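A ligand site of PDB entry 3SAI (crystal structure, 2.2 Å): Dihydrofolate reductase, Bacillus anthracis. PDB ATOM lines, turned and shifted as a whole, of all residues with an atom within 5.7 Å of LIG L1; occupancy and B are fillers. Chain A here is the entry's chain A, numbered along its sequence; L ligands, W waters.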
ATOM      1  N   MET A   9     -27.030 -19.998  16.714  1.00  0.00           N
ATOM      2  CA  MET A   9     -26.423 -20.344  17.987  1.00  0.00           C
ATOM      3  C   MET A   9     -25.678 -19.110  18.497  1.00  0.00           C
ATOM      4  O   MET A   9     -24.711 -18.670  17.882  1.00  0.00           O
ATOM      5  CB  MET A   9     -25.501 -21.557  17.845  1.00  0.00           C
ATOM      6  CG  MET A   9     -24.633 -21.846  19.058  1.00  0.00           C
ATOM      7  SD  MET A   9     -25.493 -22.295  20.602  1.00  0.00           S
ATOM      8  CE  MET A   9     -26.296 -23.843  20.134  1.00  0.00           C
ATOM      9  N   VAL A  10     -26.160 -18.558  19.614  1.00  0.00           N
ATOM     10  CA  VAL A  10     -25.662 -17.283  20.124  1.00  0.00           C
ATOM     11  C   VAL A  10     -25.797 -17.160  21.643  1.00  0.00           C
ATOM     12  O   VAL A  10     -26.712 -17.732  22.245  1.00  0.00           O
ATOM     13  CB  VAL A  10     -26.331 -16.069  19.401  1.00  0.00           C
ATOM     14  CG1 VAL A  10     -27.816 -15.965  19.752  1.00  0.00           C
ATOM     15  CG2 VAL A  10     -25.601 -14.758  19.720  1.00  0.00           C
ATOM     16  N   ALA A  11     -24.864 -16.431  22.265  1.00  0.00           N
ATOM     17  CA  ALA A  11     -24.984 -16.013  23.659  1.00  0.00           C
ATOM     18  C   ALA A  11     -24.910 -14.493  23.730  1.00  0.00           C
ATOM     19  O   ALA A  11     -23.980 -13.886  23.196  1.00  0.00           O
ATOM     20  CB  ALA A  11     -23.880 -16.637  24.484  1.00  0.00           C
ATOM     21  N   ASN A  22     -13.318  -7.491  19.325  1.00  0.00           N
ATOM     22  CA  ASN A  22     -13.151  -8.703  18.509  1.00  0.00           C
ATOM     23  C   ASN A  22     -12.928  -9.992  19.327  1.00  0.00           C
ATOM     24  O   ASN A  22     -12.220 -10.913  18.912  1.00  0.00           O
ATOM     25  CB  ASN A  22     -12.030  -8.513  17.476  1.00  0.00           C
ATOM     26  CG  ASN A  22     -12.282  -9.268  16.203  1.00  0.00           C
ATOM     27  OD1 ASN A  22     -13.420  -9.419  15.750  1.00  0.00           O
ATOM     28  ND2 ASN A  22     -11.211  -9.738  15.577  1.00  0.00           N
ATOM     29  N   ASN A  23     -13.572 -10.043  20.504  1.00  0.00           N
ATOM     30  CA  ASN A  23     -13.500 -11.192  21.392  1.00  0.00           C
ATOM     31  C   ASN A  23     -14.796 -11.305  22.198  1.00  0.00           C
ATOM     32  O   ASN A  23     -15.705 -10.479  22.044  1.00  0.00           O
ATOM     33  CB  ASN A  23     -12.275 -11.045  22.321  1.00  0.00           C
ATOM     34  CG  ASN A  23     -11.709 -12.401  22.795  1.00  0.00           C
ATOM     35  OD1 ASN A  23     -12.399 -13.422  22.788  1.00  0.00           O
ATOM     36  ND2 ASN A  23     -10.446 -12.389  23.212  1.00  0.00           N
ATOM     37  N   LEU A  24     -14.899 -12.333  23.031  1.00  0.00           N
ATOM     38  CA  LEU A  24     -16.040 -12.501  23.938  1.00  0.00           C
ATOM     39  C   LEU A  24     -15.851 -11.670  25.216  1.00  0.00           C
ATOM     40  O   LEU A  24     -14.750 -11.643  25.771  1.00  0.00           O
ATOM     41  CB  LEU A  24     -16.219 -13.974  24.299  1.00  0.00           C
ATOM     42  CG  LEU A  24     -16.548 -14.949  23.156  1.00  0.00           C
ATOM     43  CD1 LEU A  24     -16.525 -16.373  23.675  1.00  0.00           C
ATOM     44  CD2 LEU A  24     -17.902 -14.622  22.495  1.00  0.00           C
ATOM     45  N   TRP A  26     -17.072 -12.262  28.151  1.00  0.00           N
ATOM     46  CA  TRP A  26     -17.168 -13.096  29.356  1.00  0.00           C
ATOM     47  C   TRP A  26     -16.510 -14.444  29.113  1.00  0.00           C
ATOM     48  O   TRP A  26     -16.260 -14.822  27.966  1.00  0.00           O
ATOM     49  CB  TRP A  26     -18.646 -13.340  29.719  1.00  0.00           C
ATOM     50  CG  TRP A  26     -19.430 -13.880  28.540  1.00  0.00           C
ATOM     51  CD1 TRP A  26     -19.451 -15.166  28.112  1.00  0.00           C
ATOM     52  CD2 TRP A  26     -20.258 -13.138  27.634  1.00  0.00           C
ATOM     53  NE1 TRP A  26     -20.254 -15.286  26.988  1.00  0.00           N
ATOM     54  CE2 TRP A  26     -20.763 -14.047  26.682  1.00  0.00           C
ATOM     55  CE3 TRP A  26     -20.630 -11.795  27.545  1.00  0.00           C
ATOM     56  CZ2 TRP A  26     -21.620 -13.658  25.647  1.00  0.00           C
ATOM     57  CZ3 TRP A  26     -21.487 -11.406  26.511  1.00  0.00           C
ATOM     58  CH2 TRP A  26     -21.974 -12.330  25.582  1.00  0.00           C
ATOM     59  N   GLU A  31     -21.111 -22.879  29.578  1.00  0.00           N
ATOM     60  CA  GLU A  31     -21.913 -22.424  28.449  1.00  0.00           C
ATOM     61  C   GLU A  31     -21.283 -22.905  27.146  1.00  0.00           C
ATOM     62  O   GLU A  31     -21.989 -23.329  26.235  1.00  0.00           O
ATOM     63  CB  GLU A  31     -21.994 -20.899  28.454  1.00  0.00           C
ATOM     64  CG  GLU A  31     -23.239 -20.318  27.797  1.00  0.00           C
ATOM     65  CD  GLU A  31     -23.167 -20.280  26.275  1.00  0.00           C
ATOM     66  OE1 GLU A  31     -22.084 -19.990  25.724  1.00  0.00           O
ATOM     67  OE2 GLU A  31     -24.205 -20.561  25.613  1.00  0.00           O
ATOM     68  N   LEU A  32     -19.959 -22.831  27.059  1.00  0.00           N
ATOM     69  CA  LEU A  32     -19.202 -23.350  25.935  1.00  0.00           C
ATOM     70  C   LEU A  32     -19.407 -24.859  25.752  1.00  0.00           C
ATOM     71  O   LEU A  32     -19.428 -25.349  24.615  1.00  0.00           O
ATOM     72  CB  LEU A  32     -17.716 -23.017  26.120  1.00  0.00           C
ATOM     73  CG  LEU A  32     -16.680 -23.522  25.116  1.00  0.00           C
ATOM     74  CD1 LEU A  32     -16.841 -22.781  23.793  1.00  0.00           C
ATOM     75  CD2 LEU A  32     -15.245 -23.381  25.658  1.00  0.00           C
ATOM     76  N   TYR A  34     -22.184 -26.531  26.607  1.00  0.00           N
ATOM     77  CA  TYR A  34     -23.514 -26.624  26.031  1.00  0.00           C
ATOM     78  C   TYR A  34     -23.467 -26.420  24.515  1.00  0.00           C
ATOM     79  O   TYR A  34     -24.044 -27.194  23.749  1.00  0.00           O
ATOM     80  CB  TYR A  34     -24.438 -25.585  26.661  1.00  0.00           C
ATOM     81  CG  TYR A  34     -25.761 -25.417  25.965  1.00  0.00           C
ATOM     82  CD1 TYR A  34     -26.850 -26.233  26.279  1.00  0.00           C
ATOM     83  CD2 TYR A  34     -25.945 -24.416  25.005  1.00  0.00           C
ATOM     84  CE1 TYR A  34     -28.081 -26.072  25.649  1.00  0.00           C
ATOM     85  CE2 TYR A  34     -27.181 -24.240  24.367  1.00  0.00           C
ATOM     86  CZ  TYR A  34     -28.234 -25.073  24.703  1.00  0.00           C
ATOM     87  OH  TYR A  34     -29.453 -24.913  24.088  1.00  0.00           O
ATOM     88  N   VAL A  35     -22.764 -25.375  24.094  1.00  0.00           N
ATOM     89  CA  VAL A  35     -22.518 -25.101  22.676  1.00  0.00           C
ATOM     90  C   VAL A  35     -21.942 -26.332  21.973  1.00  0.00           C
ATOM     91  O   VAL A  35     -22.506 -26.783  20.968  1.00  0.00           O
ATOM     92  CB  VAL A  35     -21.571 -23.882  22.493  1.00  0.00           C
ATOM     93  CG1 VAL A  35     -21.136 -23.745  21.038  1.00  0.00           C
ATOM     94  CG2 VAL A  35     -22.245 -22.624  22.979  1.00  0.00           C
ATOM     95  N   LYS A  36     -20.850 -26.887  22.512  1.00  0.00           N
ATOM     96  CA  LYS A  36     -20.184 -28.054  21.908  1.00  0.00           C
ATOM     97  C   LYS A  36     -21.161 -29.229  21.831  1.00  0.00           C
ATOM     98  O   LYS A  36     -21.273 -29.874  20.788  1.00  0.00           O
ATOM     99  CB  LYS A  36     -18.914 -28.444  22.674  1.00  0.00           C
ATOM    100  CG  LYS A  36     -17.925 -27.290  22.843  1.00  0.00           C
ATOM    101  CD  LYS A  36     -16.672 -27.650  23.652  1.00  0.00           C
ATOM    102  CE  LYS A  36     -15.417 -27.519  22.816  1.00  0.00           C
ATOM    103  NZ  LYS A  36     -14.211 -27.293  23.661  1.00  0.00           N
ATOM    104  N   ASN A  50     -15.262 -13.679  13.152  1.00  0.00           N
ATOM    105  CA  ASN A  50     -15.527 -14.720  14.146  1.00  0.00           C
ATOM    106  C   ASN A  50     -14.530 -15.882  14.022  1.00  0.00           C
ATOM    107  O   ASN A  50     -13.949 -16.270  15.026  1.00  0.00           O
ATOM    108  CB  ASN A  50     -16.959 -15.248  14.034  1.00  0.00           C
ATOM    109  CG  ASN A  50     -17.294 -16.298  15.099  1.00  0.00           C
ATOM    110  OD1 ASN A  50     -16.676 -16.319  16.174  1.00  0.00           O
ATOM    111  ND2 ASN A  50     -18.256 -17.150  14.808  1.00  0.00           N
ATOM    112  N   ALA A  53     -10.772 -15.071  15.101  1.00  0.00           N
ATOM    113  CA  ALA A  53     -10.664 -14.948  16.547  1.00  0.00           C
ATOM    114  C   ALA A  53     -10.594 -16.326  17.214  1.00  0.00           C
ATOM    115  O   ALA A  53      -9.812 -16.532  18.152  1.00  0.00           O
ATOM    116  CB  ALA A  53     -11.822 -14.132  17.098  1.00  0.00           C
ATOM    117  N   ILE A  54     -11.412 -17.276  16.730  1.00  0.00           N
ATOM    118  CA  ILE A  54     -11.387 -18.658  17.225  1.00  0.00           C
ATOM    119  C   ILE A  54     -10.001 -19.279  16.965  1.00  0.00           C
ATOM    120  O   ILE A  54      -9.404 -19.867  17.878  1.00  0.00           O
ATOM    121  CB  ILE A  54     -12.527 -19.512  16.613  1.00  0.00           C
ATOM    122  CG1 ILE A  54     -13.891 -18.998  17.097  1.00  0.00           C
ATOM    123  CG2 ILE A  54     -12.349 -21.000  16.960  1.00  0.00           C
ATOM    124  CD1 ILE A  54     -15.081 -19.530  16.337  1.00  0.00           C
ATOM    125  N   ARG A  56      -8.754 -21.690  14.908  1.00  0.00           N
ATOM    126  CA  ARG A  56      -8.549 -23.072  14.506  1.00  0.00           C
ATOM    127  C   ARG A  56      -9.876 -23.697  14.066  1.00  0.00           C
ATOM    128  O   ARG A  56     -10.936 -23.258  14.511  1.00  0.00           O
ATOM    129  CB  ARG A  56      -7.948 -23.879  15.677  1.00  0.00           C
ATOM    130  CG  ARG A  56      -8.941 -24.122  16.822  1.00  0.00           C
ATOM    131  CD  ARG A  56      -8.295 -24.356  18.173  1.00  0.00           C
ATOM    132  NE  ARG A  56      -9.299 -24.776  19.160  1.00  0.00           N
ATOM    133  CZ  ARG A  56     -10.009 -23.966  19.936  1.00  0.00           C
ATOM    134  NH1 ARG A  56      -9.858 -22.645  19.865  1.00  0.00           N
ATOM    135  NH2 ARG A  56     -10.885 -24.469  20.797  1.00  0.00           N
ATOM    136  N   LEU A  58     -12.830 -26.167  14.378  1.00  0.00           N
ATOM    137  CA  LEU A  58     -13.428 -26.875  15.503  1.00  0.00           C
ATOM    138  C   LEU A  58     -13.733 -28.322  15.108  1.00  0.00           C
ATOM    139  O   LEU A  58     -14.313 -28.566  14.051  1.00  0.00           O
ATOM    140  CB  LEU A  58     -14.671 -26.122  16.005  1.00  0.00           C
ATOM    141  CG  LEU A  58     -14.465 -24.702  16.560  1.00  0.00           C
ATOM    142  CD1 LEU A  58     -15.757 -24.151  17.102  1.00  0.00           C
ATOM    143  CD2 LEU A  58     -13.368 -24.614  17.630  1.00  0.00           C
ATOM    144  N   ILE A  98     -25.720 -21.240  12.455  1.00  0.00           N
ATOM    145  CA  ILE A  98     -25.162 -19.925  12.251  1.00  0.00           C
ATOM    146  C   ILE A  98     -24.546 -19.533  13.587  1.00  0.00           C
ATOM    147  O   ILE A  98     -25.239 -19.376  14.584  1.00  0.00           O
ATOM    148  CB  ILE A  98     -26.238 -18.896  11.780  1.00  0.00           C
ATOM    149  CG1 ILE A  98     -27.103 -19.479  10.653  1.00  0.00           C
ATOM    150  CG2 ILE A  98     -25.594 -17.583  11.360  1.00  0.00           C
ATOM    151  CD1 ILE A  98     -26.350 -19.892   9.368  1.00  0.00           C
ATOM    152  N   PHE A  99     -23.222 -19.395  13.570  1.00  0.00           N
ATOM    153  CA  PHE A  99     -22.408 -19.290  14.775  1.00  0.00           C
ATOM    154  C   PHE A  99     -21.896 -17.861  15.022  1.00  0.00           C
ATOM    155  O   PHE A  99     -21.130 -17.641  15.961  1.00  0.00           O
ATOM    156  CB  PHE A  99     -21.229 -20.268  14.627  1.00  0.00           C
ATOM    157  CG  PHE A  99     -20.615 -20.706  15.928  1.00  0.00           C
ATOM    158  CD1 PHE A  99     -21.372 -21.360  16.902  1.00  0.00           C
ATOM    159  CD2 PHE A  99     -19.249 -20.513  16.153  1.00  0.00           C
ATOM    160  CE1 PHE A  99     -20.796 -21.781  18.091  1.00  0.00           C
ATOM    161  CE2 PHE A  99     -18.664 -20.928  17.361  1.00  0.00           C
ATOM    162  CZ  PHE A  99     -19.444 -21.565  18.329  1.00  0.00           C
ATOM    163  N   GLY A 100     -22.311 -16.911  14.188  1.00  0.00           N
ATOM    164  CA  GLY A 100     -21.891 -15.511  14.339  1.00  0.00           C
ATOM    165  C   GLY A 100     -20.701 -15.099  13.497  1.00  0.00           C
ATOM    166  O   GLY A 100     -20.181 -15.907  12.737  1.00  0.00           O
ATOM    167  N   TYR A 105     -25.041 -13.016  11.465  1.00  0.00           N
ATOM    168  CA  TYR A 105     -26.410 -13.147  11.978  1.00  0.00           C
ATOM    169  C   TYR A 105     -27.383 -12.292  11.174  1.00  0.00           C
ATOM    170  O   TYR A 105     -28.466 -12.745  10.840  1.00  0.00           O
ATOM    171  CB  TYR A 105     -26.521 -12.779  13.466  1.00  0.00           C
ATOM    172  CG  TYR A 105     -25.842 -13.714  14.446  1.00  0.00           C
ATOM    173  CD1 TYR A 105     -26.049 -15.088  14.391  1.00  0.00           C
ATOM    174  CD2 TYR A 105     -25.001 -13.216  15.444  1.00  0.00           C
ATOM    175  CE1 TYR A 105     -25.433 -15.941  15.298  1.00  0.00           C
ATOM    176  CE2 TYR A 105     -24.384 -14.054  16.351  1.00  0.00           C
ATOM    177  CZ  TYR A 105     -24.617 -15.427  16.265  1.00  0.00           C
ATOM    178  OH  TYR A 105     -24.001 -16.272  17.161  1.00  0.00           O
ATOM    179  N   TYR A 116     -31.215 -20.945  19.186  1.00  0.00           N
ATOM    180  CA  TYR A 116     -30.621 -21.375  20.452  1.00  0.00           C
ATOM    181  C   TYR A 116     -29.896 -20.174  21.041  1.00  0.00           C
ATOM    182  O   TYR A 116     -28.810 -19.785  20.572  1.00  0.00           O
ATOM    183  CB  TYR A 116     -29.628 -22.509  20.254  1.00  0.00           C
ATOM    184  CG  TYR A 116     -30.163 -23.768  19.633  1.00  0.00           C
ATOM    185  CD1 TYR A 116     -30.508 -23.814  18.273  1.00  0.00           C
ATOM    186  CD2 TYR A 116     -30.292 -24.943  20.374  1.00  0.00           C
ATOM    187  CE1 TYR A 116     -30.991 -24.970  17.692  1.00  0.00           C
ATOM    188  CE2 TYR A 116     -30.782 -26.120  19.797  1.00  0.00           C
ATOM    189  CZ  TYR A 116     -31.116 -26.117  18.457  1.00  0.00           C
ATOM    190  OH  TYR A 116     -31.586 -27.261  17.867  1.00  0.00           O
ATOM    191  N   THR A 118     -28.563 -18.143  24.491  1.00  0.00           N
ATOM    192  CA  THR A 118     -28.238 -18.032  25.898  1.00  0.00           C
ATOM    193  C   THR A 118     -28.338 -16.566  26.294  1.00  0.00           C
ATOM    194  O   THR A 118     -27.772 -15.681  25.639  1.00  0.00           O
ATOM    195  CB  THR A 118     -26.824 -18.594  26.193  1.00  0.00           C
ATOM    196  OG1 THR A 118     -26.731 -19.946  25.731  1.00  0.00           O
ATOM    197  CG2 THR A 118     -26.521 -18.522  27.708  1.00  0.00           C
HETATM  198  N1  LIG L   1     -23.192 -19.269  20.909  1.00  0.00           N
HETATM  199  C1  LIG L   1     -23.202 -19.421  22.242  1.00  0.00           C
HETATM  200  N2  LIG L   1     -22.113 -19.172  22.989  1.00  0.00           N
HETATM  201  C2  LIG L   1     -20.965 -18.739  22.446  1.00  0.00           C
HETATM  202  C3  LIG L   1     -20.928 -18.568  21.066  1.00  0.00           C
HETATM  203  C4  LIG L   1     -22.061 -18.835  20.301  1.00  0.00           C
HETATM  204  C5  LIG L   1     -18.970 -19.747  23.597  1.00  0.00           C
HETATM  205  C6  LIG L   1     -12.944 -15.466  20.558  1.00  0.00           C
HETATM  206  N3  LIG L   1     -24.278 -19.838  22.857  1.00  0.00           N
HETATM  207  N4  LIG L   1     -22.042 -18.656  18.976  1.00  0.00           N
HETATM  208  C7  LIG L   1     -18.678 -17.706  19.937  1.00  0.00           C
HETATM  209  C8  LIG L   1     -19.721 -18.106  20.447  1.00  0.00           C
HETATM  210  C9  LIG L   1     -13.800 -23.033  22.037  1.00  0.00           C
HETATM  211  C10 LIG L   1     -15.516 -23.463  20.523  1.00  0.00           C
HETATM  212  C11 LIG L   1     -13.894 -21.665  21.782  1.00  0.00           C
HETATM  213  C12 LIG L   1     -15.649 -22.106  20.222  1.00  0.00           C
HETATM  214  C13 LIG L   1     -15.043 -17.092  20.035  1.00  0.00           C
HETATM  215  C14 LIG L   1     -16.108 -19.259  20.102  1.00  0.00           C
HETATM  216  C15 LIG L   1     -13.808 -19.012  20.789  1.00  0.00           C
HETATM  217  C16 LIG L   1     -19.800 -18.488  23.404  1.00  0.00           C
HETATM  218  C17 LIG L   1     -17.443 -17.232  19.284  1.00  0.00           C
HETATM  219  N5  LIG L   1     -14.610 -23.879  21.410  1.00  0.00           N
HETATM  220  O1  LIG L   1     -12.723 -16.888  20.729  1.00  0.00           O
HETATM  221  C18 LIG L   1     -16.173 -17.886  19.824  1.00  0.00           C
HETATM  222  C19 LIG L   1     -13.845 -17.648  20.513  1.00  0.00           C
HETATM  223  C20 LIG L   1     -14.821 -21.190  20.864  1.00  0.00           C
HETATM  224  C21 LIG L   1     -14.921 -19.815  20.589  1.00  0.00           C
HETATM  225  P1  LG2 L   2     -18.324 -11.478  11.688  1.00  0.00           P
HETATM  226  O1  LG2 L   2     -19.779 -11.345  11.466  1.00  0.00           O
HETATM  227  O2  LG2 L   2     -17.981 -12.714  12.434  1.00  0.00           O
HETATM  228  O3  LG2 L   2     -17.533 -11.455  10.294  1.00  0.00           O
HETATM  229  C1  LG2 L   2     -17.567 -10.295   9.493  1.00  0.00           C
HETATM  230  C2  LG2 L   2     -16.994 -10.707   8.150  1.00  0.00           C
HETATM  231  O4  LG2 L   2     -17.880 -11.597   7.492  1.00  0.00           O
HETATM  232  C3  LG2 L   2     -16.781  -9.590   7.152  1.00  0.00           C
HETATM  233  O5  LG2 L   2     -15.622  -8.847   7.414  1.00  0.00           O
HETATM  234  C4  LG2 L   2     -16.706 -10.380   5.864  1.00  0.00           C
HETATM  235  O6  LG2 L   2     -15.447 -11.025   5.709  1.00  0.00           O
HETATM  236  C5  LG2 L   2     -17.757 -11.448   6.105  1.00  0.00           C
HETATM  237  N1  LG2 L   2     -19.028 -10.971   5.527  1.00  0.00           N
HETATM  238  C6  LG2 L   2     -19.894 -10.058   6.075  1.00  0.00           C
HETATM  239  N2  LG2 L   2     -20.934  -9.900   5.233  1.00  0.00           N
HETATM  240  C7  LG2 L   2     -20.742 -10.684   4.148  1.00  0.00           C
HETATM  241  C8  LG2 L   2     -21.474 -10.902   2.997  1.00  0.00           C
HETATM  242  N3  LG2 L   2     -22.622 -10.254   2.798  1.00  0.00           N
HETATM  243  N4  LG2 L   2     -21.018 -11.798   2.050  1.00  0.00           N
HETATM  244  C9  LG2 L   2     -19.831 -12.470   2.241  1.00  0.00           C
HETATM  245  N5  LG2 L   2     -19.106 -12.251   3.384  1.00  0.00           N
HETATM  246  C10 LG2 L   2     -19.546 -11.370   4.330  1.00  0.00           C
HETATM  247  O7  LG2 L   2     -17.778 -10.162  12.448  1.00  0.00           O
HETATM  248  P2  LG2 L   2     -18.467  -9.210  13.542  1.00  0.00           P
HETATM  249  O8  LG2 L   2     -17.505  -8.109  13.796  1.00  0.00           O
HETATM  250  O9  LG2 L   2     -19.852  -8.907  13.089  1.00  0.00           O
HETATM  251  O10 LG2 L   2     -18.607 -10.174  14.828  1.00  0.00           O
HETATM  252  C11 LG2 L   2     -17.438 -10.528  15.537  1.00  0.00           C
HETATM  253  C12 LG2 L   2     -17.631 -10.238  17.024  1.00  0.00           C
HETATM  254  O11 LG2 L   2     -18.745 -10.964  17.561  1.00  0.00           O
HETATM  255  C13 LG2 L   2     -16.423 -10.694  17.811  1.00  0.00           C
HETATM  256  O12 LG2 L   2     -16.332  -9.827  18.926  1.00  0.00           O
HETATM  257  C14 LG2 L   2     -16.796 -12.085  18.274  1.00  0.00           C
HETATM  258  O13 LG2 L   2     -16.085 -12.469  19.431  1.00  0.00           O
HETATM  259  C15 LG2 L   2     -18.287 -11.896  18.543  1.00  0.00           C
HETATM  260  N6  LG2 L   2     -19.080 -13.129  18.492  1.00  0.00           N
HETATM  261  C16 LG2 L   2     -19.867 -13.417  19.579  1.00  0.00           C
HETATM  262  C17 LG2 L   2     -20.659 -14.558  19.598  1.00  0.00           C
HETATM  263  C18 LG2 L   2     -21.544 -14.858  20.779  1.00  0.00           C
HETATM  264  O14 LG2 L   2     -22.553 -15.833  20.664  1.00  0.00           O
HETATM  265  N7  LG2 L   2     -21.380 -14.182  21.912  1.00  0.00           N
HETATM  266  C19 LG2 L   2     -20.655 -15.404  18.484  1.00  0.00           C
HETATM  267  C20 LG2 L   2     -19.850 -15.096  17.383  1.00  0.00           C
HETATM  268  C21 LG2 L   2     -19.066 -13.941  17.398  1.00  0.00           C
HETATM  269  P3  LG2 L   2     -14.249 -10.357   4.849  1.00  0.00           P
HETATM  270  O15 LG2 L   2     -13.857  -9.065   5.528  1.00  0.00           O
HETATM  271  O16 LG2 L   2     -13.051 -11.273   4.794  1.00  0.00           O
HETATM  272  O17 LG2 L   2     -14.764 -10.106   3.455  1.00  0.00           O
HETATM  273  O   HOH W   1     -20.436 -17.834  26.723  1.00  0.00           O
HETATM  274  O   HOH W   2     -14.898 -14.744  17.838  1.00  0.00           O
HETATM  275  O   HOH W   3     -27.493 -20.937  23.330  1.00  0.00           O
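A nitrogen (N3) of LIG L1 lies within hydrogen-bond range of the side-chain carboxylate (OE2) of Glu 31. O of Met 9 lies within hydrogen-bond range of N4 of LIG L1 (2.9 Å). SD of Met 9 sits at hydrogen-bond distance from N3 of LIG L1, 3.5 Å away. N1 of LIG L1 lies close to N of Val 10 (3.3 Å). O of Val 10 sits at hydrogen-bond distance from N3 of LIG L1, at 3.3 Å. O of Phe 99 is in hydrogen-bond range of N4 of LIG L1, at 3.3 Å. N of Asn 23 lies within hydrogen-bond range of O12 of LG2 L2 (3.2 Å). An oxygen (O12) of LG2 L2 sits at hydrogen-bond distance from the backbone carbonyl oxygen (O) of Asn 23 (3.2 Å). N of Asn 50 lies within hydrogen-bond range of O2 of LG2 L2 (3.0 Å). N of Ala 11 is in hydrogen-bond range of O14 of LG2 L2 (2.9 Å). N7 of LG2 L2 lies within hydrogen-bond range of O of Ala 11, 2.9 Å away.
An oxygen (O14) of LG2 L2 lies close to a nitrogen (N4) of LIG L1.
The backbone carbonyl oxygen (O) of Met 9 sits at hydrogen-bond distance from the side-chain hydroxyl (OH) of Tyr 105 (2.6 Å). N of Met 9 sits at hydrogen-bond distance from O of Ile 98 (2.9 Å). O of Val 10 sits at hydrogen-bond distance from N of Thr 118. The backbone carbonyl oxygen (O) of Phe 99 lies within hydrogen-bond range of the side-chain amide nitrogen (ND2) of Asn 50, 3.1 Å away. OH of Tyr 105 sits close to O of Phe 99 (3.4 Å). The backbone carbonyl oxygen (O) of Gly 100 is in hydrogen-bond range of the side-chain amide nitrogen (ND2) of Asn 50 (3.1 Å). The guanidinium group of Arg 56 is in hydrogen-bond range of the backbone carbonyl oxygen of Ile 54, 3.4 Å away. The side-chain hydroxyl of Tyr 105 lies close to the backbone NH of Gly 100, at 3.5 Å.
N of Ala 11 touches C1 of LIG L1, at 3.4 Å. Asn 23 touches LIG L1. CD1 of Leu 24 touches C16 of LIG L1, at 3.9 Å. Leu 32 touches LIG L1 (CD1 to N5, 3.4 Å). Val 35 touches LIG L1 (CG2 to C1, 3.4 Å). Lys 36 touches LIG L1. OD1 of Asn 50 touches C17 of LIG L1, 3.3 Å away. CB of Ala 53 touches C6 of LIG L1 (3.9 Å). Ile 54 touches LIG L1. Arg 56 touches LIG L1 (NH2 to C9, 3.5 Å). Leu 58 touches LIG L1 (CD1 to C10, 3.5 Å). OH of Tyr 105 touches N4 of LIG L1, at 3.6 Å. Thr 118 touches LIG L1 (OG1 to N3, 3.8 Å). Hydrophobic or aromatic side chains that line LIG L1: Met 9, Ala 11, Leu 24, Leu 32, Val 35, Ala 53, Ile 54, Leu 58 and Phe 99. Of the 23 residues printed, 17 come within 4 Å of LIG L1. Along chain A the residues within 4 Å of LIG L1 span positions 9 to 118. The nearest printed residue that does not touch LIG L1 is Trp 26 (4.8 Å).
Water W2 bridges OD1 of Asn 50 (2.9 Å) and O13 of LG2 L2 (3.0 Å). Water W1 bridges NE1 of Trp 26 (2.6 Å) and OE1 of Glu 31 (2.9 Å).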
